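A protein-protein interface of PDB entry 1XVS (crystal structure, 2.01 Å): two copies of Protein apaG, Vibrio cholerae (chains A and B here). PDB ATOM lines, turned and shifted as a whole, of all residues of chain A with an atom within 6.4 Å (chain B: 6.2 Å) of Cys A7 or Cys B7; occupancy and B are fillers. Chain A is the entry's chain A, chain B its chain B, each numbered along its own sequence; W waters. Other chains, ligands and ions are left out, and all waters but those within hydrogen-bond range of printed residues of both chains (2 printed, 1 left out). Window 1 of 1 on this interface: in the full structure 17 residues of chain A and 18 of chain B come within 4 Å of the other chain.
Water W2 bridges the side-chain amino group of Lys B9 (3.0 Å) and the backbone NH of Cys A7 (3.3 Å).
Water W1 bridges NZ of Lys A9 (3.1 Å) and N of Cys B7 (3.3 Å).
The backbone carbonyl oxygen (O) of Cys A7 lies within hydrogen-bond range of the backbone NH (N) of Leu A39.
The backbone carbonyl oxygen (O) of Lys A37 sits at hydrogen-bond distance from the backbone NH (N) of Lys A9 (2.9 Å).
The side-chain amide oxygen (OD1) of Asn A38 is in hydrogen-bond range of the side-chain hydroxyl (OG) of Ser A40 (2.6 Å).
The backbone carbonyl oxygen (O) of Cys B7 sits at hydrogen-bond distance from the backbone NH (N) of Leu B39 (2.9 Å).
The backbone NH (N) of Lys B37 lies within hydrogen-bond range of the backbone carbonyl oxygen (O) of Lys B9 (2.9 Å).
OG of Ser B40 sits at hydrogen-bond distance from OD1 of Asn B38 (2.7 Å).
Among the printed residues, pairs that only touch across the chains: Ser A4 with Lys B9 (3.7 Å), Cys A7 with Ile B8 (3.9 Å), Cys A7 with Leu B39 (3.8 Å), Ile A8 with Ser B4 (3.6 Å), Lys A9 with Ser B4 (3.4 Å), Lys A9 with Ser B40 (3.7 Å), Leu A39 with Leu B39 (3.9 Å) and Ser A40 with Lys B9 (3.8 Å).
Of the 11 printed residues of chain A, 6 touch a printed residue of chain B.
Among the printed residues, 12 pairs touch across the chains.
Ser A4 touches Lys B9, and with the chains exchanged Lys A9 touches Ser B4.
Cys A7 touches Ile B8, but with the chains exchanged Ile A8 does not touch Cys B7 (4.02 Å).
Cys A7 touches Leu B39, but with the chains exchanged Leu A39 does not touch Cys B7 (4.1 Å).
Lys A9 touches Leu B39, and with the chains exchanged Leu A39 touches Lys B9.
11 positions are printed for both chains.
Of the 12 pairs that touch across the chains among the printed residues, 10 have their exchanged pair printed and touching as well.
The backbone carbonyl oxygen (O) of Ile B8 lies within hydrogen-bond range of the side-chain hydroxyl (OG) of Ser A4 (3.2 Å).
The side-chain sulfur (SG) of Cys B7 lies close to the side-chain sulfur (SG) of Cys A7.
NZ of Lys A9 sits at hydrogen-bond distance from O of Leu B39, 2.7 Å away.
NZ of Lys B9 is in hydrogen-bond range of O of Leu A39 (2.6 Å).
Of chain B, only Cys B7, Ile B8 and Leu B39 come within 4 Å of Cys A7.
Of the printed residues of chain A, Cys B7 touches Cys A7.
Of the printed residues of chain B, Leu A39 touches Lys B9 and Leu B39.
Of the printed residues of chain A, Ile B8 touches Ser A4 and Cys A7.
Of the printed residues of chain B, Ser A40 touches Lys B9 (3.8 Å).
Printed residues of chain B within 4 Å of Ser A4: Ile B8 and Lys B9.
Printed residues of chain A within 4 Å of Lys B9: Ser A4, Leu A39 and Ser A40.
Leu A5 touches none of the printed residues of chain B.
Leu B5 touches none of the printed residues of chain A.
The nearest residue of chain B that does not touch Cys A7 is Lys B9 (4.6 Å).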
ATOM      1  N   SER A   4      16.737  -0.398  28.439  1.00  0.00           N
ATOM      2  CA  SER A   4      15.354  -0.566  27.944  1.00  0.00           C
ATOM      3  C   SER A   4      15.343  -1.900  27.200  1.00  0.00           C
ATOM      4  O   SER A   4      16.377  -2.242  26.543  1.00  0.00           O
ATOM      5  CB  SER A   4      15.089   0.524  26.873  1.00  0.00           C
ATOM      6  OG  SER A   4      14.315   1.518  27.445  1.00  0.00           O
ATOM      7  N   LEU A   5      14.236  -2.642  27.181  1.00  0.00           N
ATOM      8  CA  LEU A   5      14.219  -3.920  26.332  1.00  0.00           C
ATOM      9  C   LEU A   5      14.375  -3.567  24.840  1.00  0.00           C
ATOM     10  O   LEU A   5      14.056  -2.461  24.468  1.00  0.00           O
ATOM     11  CB  LEU A   5      12.887  -4.647  26.543  1.00  0.00           C
ATOM     12  CG  LEU A   5      12.630  -5.363  27.879  1.00  0.00           C
ATOM     13  CD1 LEU A   5      11.402  -6.205  27.683  1.00  0.00           C
ATOM     14  CD2 LEU A   5      13.829  -6.240  28.236  1.00  0.00           C
ATOM     15  N   PRO A   6      14.909  -4.459  24.001  1.00  0.00           N
ATOM     16  CA  PRO A   6      15.005  -4.129  22.560  1.00  0.00           C
ATOM     17  C   PRO A   6      13.675  -3.628  21.959  1.00  0.00           C
ATOM     18  O   PRO A   6      12.658  -4.153  22.236  1.00  0.00           O
ATOM     19  CB  PRO A   6      15.489  -5.431  21.887  1.00  0.00           C
ATOM     20  CG  PRO A   6      16.081  -6.232  22.970  1.00  0.00           C
ATOM     21  CD  PRO A   6      15.551  -5.768  24.328  1.00  0.00           C
ATOM     22  N   CYS A   7      13.694  -2.534  21.232  1.00  0.00           N
ATOM     23  CA  CYS A   7      12.432  -2.031  20.684  1.00  0.00           C
ATOM     24  C   CYS A   7      11.980  -2.830  19.428  1.00  0.00           C
ATOM     25  O   CYS A   7      12.713  -2.895  18.424  1.00  0.00           O
ATOM     26  CB  CYS A   7      12.610  -0.547  20.321  1.00  0.00           C
ATOM     27  SG  CYS A   7      12.397   0.740  21.678  1.00  0.00           S
ATOM     28  N   ILE A   8      10.807  -3.442  19.530  1.00  0.00           N
ATOM     29  CA  ILE A   8      10.202  -4.184  18.471  1.00  0.00           C
ATOM     30  C   ILE A   8       8.931  -3.421  18.095  1.00  0.00           C
ATOM     31  O   ILE A   8       8.070  -3.262  19.009  1.00  0.00           O
ATOM     32  CB  ILE A   8       9.781  -5.562  19.037  1.00  0.00           C
ATOM     33  CG1 ILE A   8      10.985  -6.421  19.516  1.00  0.00           C
ATOM     34  CG2 ILE A   8       8.989  -6.398  17.954  1.00  0.00           C
ATOM     35  CD1 ILE A   8      12.316  -6.374  18.564  1.00  0.00           C
ATOM     36  N   LYS A   9       8.758  -2.962  16.823  1.00  0.00           N
ATOM     37  CA  LYS A   9       7.526  -2.264  16.439  1.00  0.00           C
ATOM     38  C   LYS A   9       6.665  -3.236  15.651  1.00  0.00           C
ATOM     39  O   LYS A   9       7.080  -3.818  14.712  1.00  0.00           O
ATOM     40  CB  LYS A   9       7.838  -0.967  15.654  1.00  0.00           C
ATOM     41  CG  LYS A   9       6.636  -0.040  15.194  1.00  0.00           C
ATOM     42  CD  LYS A   9       7.179   1.429  14.686  1.00  0.00           C
ATOM     43  CE  LYS A   9       8.343   2.068  15.622  1.00  0.00           C
ATOM     44  NZ  LYS A   9       8.878   3.585  15.586  1.00  0.00           N
ATOM     45  N   LYS A  37       9.296  -4.971  12.990  1.00  0.00           N
ATOM     46  CA  LYS A  37      10.508  -4.150  12.699  1.00  0.00           C
ATOM     47  C   LYS A  37      11.400  -4.120  13.939  1.00  0.00           C
ATOM     48  O   LYS A  37      10.907  -3.814  15.079  1.00  0.00           O
ATOM     49  CB  LYS A  37      10.074  -2.708  12.331  1.00  0.00           C
ATOM     50  CG  LYS A  37       8.907  -2.595  11.365  1.00  0.00           C
ATOM     51  CD  LYS A  37       8.455  -1.084  11.333  1.00  0.00           C
ATOM     52  CE  LYS A  37       7.556  -0.661  10.072  1.00  0.00           C
ATOM     53  NZ  LYS A  37       8.168  -0.747   8.663  1.00  0.00           N
ATOM     54  N   ASN A  38      12.663  -4.480  13.771  1.00  0.00           N
ATOM     55  CA  ASN A  38      13.568  -4.508  14.844  1.00  0.00           C
ATOM     56  C   ASN A  38      14.126  -3.106  14.851  1.00  0.00           C
ATOM     57  O   ASN A  38      14.787  -2.678  13.875  1.00  0.00           O
ATOM     58  CB  ASN A  38      14.681  -5.579  14.613  1.00  0.00           C
ATOM     59  CG  ASN A  38      15.724  -5.630  15.707  1.00  0.00           C
ATOM     60  OD1 ASN A  38      15.661  -4.865  16.679  1.00  0.00           O
ATOM     61  ND2 ASN A  38      16.687  -6.579  15.587  1.00  0.00           N
ATOM     62  N   LEU A  39      13.763  -2.350  15.887  1.00  0.00           N
ATOM     63  CA  LEU A  39      14.357  -1.028  16.070  1.00  0.00           C
ATOM     64  C   LEU A  39      15.458  -0.957  17.072  1.00  0.00           C
ATOM     65  O   LEU A  39      15.792   0.128  17.552  1.00  0.00           O
ATOM     66  CB  LEU A  39      13.313   0.052  16.449  1.00  0.00           C
ATOM     67  CG  LEU A  39      11.969   0.233  15.784  1.00  0.00           C
ATOM     68  CD1 LEU A  39      11.204   1.472  16.277  1.00  0.00           C
ATOM     69  CD2 LEU A  39      12.007   0.129  14.255  1.00  0.00           C
ATOM     70  N   SER A  40      16.114  -2.053  17.367  1.00  0.00           N
ATOM     71  CA  SER A  40      17.135  -2.057  18.459  1.00  0.00           C
ATOM     72  C   SER A  40      18.526  -2.021  17.816  1.00  0.00           C
ATOM     73  O   SER A  40      18.616  -1.893  16.589  1.00  0.00           O
ATOM     74  CB  SER A  40      17.010  -3.299  19.316  1.00  0.00           C
ATOM     75  OG  SER A  40      17.426  -4.369  18.508  1.00  0.00           O
ATOM     76  N   PHE A 110      12.845 -12.216  25.930  1.00  0.00           N
ATOM     77  CA  PHE A 110      11.999 -11.032  26.249  1.00  0.00           C
ATOM     78  C   PHE A 110      10.635 -11.174  25.592  1.00  0.00           C
ATOM     79  O   PHE A 110      10.513 -11.800  24.494  1.00  0.00           O
ATOM     80  CB  PHE A 110      12.709  -9.679  26.042  1.00  0.00           C
ATOM     81  CG  PHE A 110      12.962  -9.294  24.602  1.00  0.00           C
ATOM     82  CD1 PHE A 110      14.065  -9.761  23.912  1.00  0.00           C
ATOM     83  CD2 PHE A 110      12.140  -8.381  23.985  1.00  0.00           C
ATOM     84  CE1 PHE A 110      14.320  -9.373  22.604  1.00  0.00           C
ATOM     85  CE2 PHE A 110      12.324  -8.034  22.650  1.00  0.00           C
ATOM     86  CZ  PHE A 110      13.448  -8.513  21.955  1.00  0.00           C
ATOM     87  N   SER B   4       2.018  -2.136  18.894  1.00  0.00           N
ATOM     88  CA  SER B   4       2.963  -2.281  19.983  1.00  0.00           C
ATOM     89  C   SER B   4       2.976  -0.944  20.652  1.00  0.00           C
ATOM     90  O   SER B   4       2.699   0.061  20.014  1.00  0.00           O
ATOM     91  CB  SER B   4       4.431  -2.429  19.572  1.00  0.00           C
ATOM     92  OG  SER B   4       4.633  -2.470  18.223  1.00  0.00           O
ATOM     93  N   LEU B   5       3.339  -0.913  21.923  1.00  0.00           N
ATOM     94  CA  LEU B   5       3.430   0.383  22.640  1.00  0.00           C
ATOM     95  C   LEU B   5       4.579   1.211  22.039  1.00  0.00           C
ATOM     96  O   LEU B   5       5.532   0.653  21.557  1.00  0.00           O
ATOM     97  CB  LEU B   5       3.732   0.121  24.126  1.00  0.00           C
ATOM     98  CG  LEU B   5       2.602  -0.593  24.930  1.00  0.00           C
ATOM     99  CD1 LEU B   5       3.082  -0.883  26.302  1.00  0.00           C
ATOM    100  CD2 LEU B   5       1.307   0.252  25.021  1.00  0.00           C
ATOM    101  N   PRO B   6       4.495   2.535  22.150  1.00  0.00           N
ATOM    102  CA  PRO B   6       5.529   3.408  21.637  1.00  0.00           C
ATOM    103  C   PRO B   6       6.856   2.918  22.150  1.00  0.00           C
ATOM    104  O   PRO B   6       7.040   2.637  23.308  1.00  0.00           O
ATOM    105  CB  PRO B   6       5.195   4.814  22.223  1.00  0.00           C
ATOM    106  CG  PRO B   6       3.746   4.703  22.602  1.00  0.00           C
ATOM    107  CD  PRO B   6       3.342   3.269  22.752  1.00  0.00           C
ATOM    108  N   CYS B   7       7.790   2.824  21.238  1.00  0.00           N
ATOM    109  CA  CYS B   7       9.169   2.545  21.603  1.00  0.00           C
ATOM    110  C   CYS B   7       9.887   3.776  22.225  1.00  0.00           C
ATOM    111  O   CYS B   7      10.124   4.807  21.514  1.00  0.00           O
ATOM    112  CB  CYS B   7       9.911   2.141  20.361  1.00  0.00           C
ATOM    113  SG  CYS B   7       9.563   0.382  19.823  1.00  0.00           S
ATOM    114  N   ILE B   8      10.331   3.581  23.462  1.00  0.00           N
ATOM    115  CA  ILE B   8      11.029   4.551  24.322  1.00  0.00           C
ATOM    116  C   ILE B   8      12.434   3.841  24.619  1.00  0.00           C
ATOM    117  O   ILE B   8      12.454   2.730  25.171  1.00  0.00           O
ATOM    118  CB  ILE B   8      10.287   4.608  25.708  1.00  0.00           C
ATOM    119  CG1 ILE B   8       8.876   5.121  25.633  1.00  0.00           C
ATOM    120  CG2 ILE B   8      10.995   5.563  26.676  1.00  0.00           C
ATOM    121  CD1 ILE B   8       8.696   6.313  24.531  1.00  0.00           C
ATOM    122  N   LYS B   9      13.570   4.414  24.212  1.00  0.00           N
ATOM    123  CA  LYS B   9      14.891   3.855  24.495  1.00  0.00           C
ATOM    124  C   LYS B   9      15.441   4.595  25.732  1.00  0.00           C
ATOM    125  O   LYS B   9      15.545   5.823  25.698  1.00  0.00           O
ATOM    126  CB  LYS B   9      15.766   4.173  23.251  1.00  0.00           C
ATOM    127  CG  LYS B   9      17.060   3.396  23.100  1.00  0.00           C
ATOM    128  CD  LYS B   9      17.590   3.284  21.555  1.00  0.00           C
ATOM    129  CE  LYS B   9      16.620   2.366  20.613  1.00  0.00           C
ATOM    130  NZ  LYS B   9      17.097   1.643  19.270  1.00  0.00           N
ATOM    131  N   LYS B  37      14.958   8.503  24.884  1.00  0.00           N
ATOM    132  CA  LYS B  37      14.727   8.770  23.480  1.00  0.00           C
ATOM    133  C   LYS B  37      13.330   8.239  22.991  1.00  0.00           C
ATOM    134  O   LYS B  37      13.035   7.046  23.183  1.00  0.00           O
ATOM    135  CB  LYS B  37      15.876   8.115  22.626  1.00  0.00           C
ATOM    136  CG  LYS B  37      17.321   8.286  23.284  1.00  0.00           C
ATOM    137  CD  LYS B  37      18.523   7.374  22.571  1.00  0.00           C
ATOM    138  CE  LYS B  37      20.010   7.833  23.037  1.00  0.00           C
ATOM    139  NZ  LYS B  37      20.753   8.654  21.908  1.00  0.00           N
ATOM    140  N   ASN B  38      12.517   9.114  22.355  1.00  0.00           N
ATOM    141  CA  ASN B  38      11.318   8.723  21.687  1.00  0.00           C
ATOM    142  C   ASN B  38      11.630   8.210  20.275  1.00  0.00           C
ATOM    143  O   ASN B  38      12.049   8.978  19.377  1.00  0.00           O
ATOM    144  CB  ASN B  38      10.347   9.896  21.714  1.00  0.00           C
ATOM    145  CG  ASN B  38       8.989   9.513  21.321  1.00  0.00           C
ATOM    146  OD1 ASN B  38       8.767   8.394  20.806  1.00  0.00           O
ATOM    147  ND2 ASN B  38       8.083  10.488  21.362  1.00  0.00           N
ATOM    148  N   LEU B  39      11.556   6.906  20.129  1.00  0.00           N
ATOM    149  CA  LEU B  39      11.589   6.200  18.878  1.00  0.00           C
ATOM    150  C   LEU B  39      10.247   5.837  18.314  1.00  0.00           C
ATOM    151  O   LEU B  39      10.216   5.059  17.352  1.00  0.00           O
ATOM    152  CB  LEU B  39      12.419   4.901  18.906  1.00  0.00           C
ATOM    153  CG  LEU B  39      13.730   5.033  19.636  1.00  0.00           C
ATOM    154  CD1 LEU B  39      14.192   3.588  19.824  1.00  0.00           C
ATOM    155  CD2 LEU B  39      14.687   5.929  18.825  1.00  0.00           C
ATOM    156  N   SER B  40       9.158   6.435  18.778  1.00  0.00           N
ATOM    157  CA  SER B  40       7.913   6.127  18.124  1.00  0.00           C
ATOM    158  C   SER B  40       7.592   7.267  17.163  1.00  0.00           C
ATOM    159  O   SER B  40       8.415   8.155  17.015  1.00  0.00           O
ATOM    160  CB  SER B  40       6.829   6.018  19.118  1.00  0.00           C
ATOM    161  OG  SER B  40       6.539   7.318  19.615  1.00  0.00           O
ATOM    162  N   PHE B 110       1.020   4.181  29.607  1.00  0.00           N
ATOM    163  CA  PHE B 110       1.836   2.995  29.339  1.00  0.00           C
ATOM    164  C   PHE B 110       3.067   3.035  30.249  1.00  0.00           C
ATOM    165  O   PHE B 110       3.647   4.135  30.540  1.00  0.00           O
ATOM    166  CB  PHE B 110       2.074   2.849  27.783  1.00  0.00           C
ATOM    167  CG  PHE B 110       3.070   3.823  27.179  1.00  0.00           C
ATOM    168  CD1 PHE B 110       2.671   5.060  26.679  1.00  0.00           C
ATOM    169  CD2 PHE B 110       4.379   3.446  27.035  1.00  0.00           C
ATOM    170  CE1 PHE B 110       3.600   5.945  26.130  1.00  0.00           C
ATOM    171  CE2 PHE B 110       5.310   4.304  26.475  1.00  0.00           C
ATOM    172  CZ  PHE B 110       4.894   5.552  25.998  1.00  0.00           C
HETATM  173  O   HOH W   1       7.142   2.739  18.053  1.00  0.00           O
HETATM  174  O   HOH W   2      16.145  -0.332  21.333  1.00  0.00           O
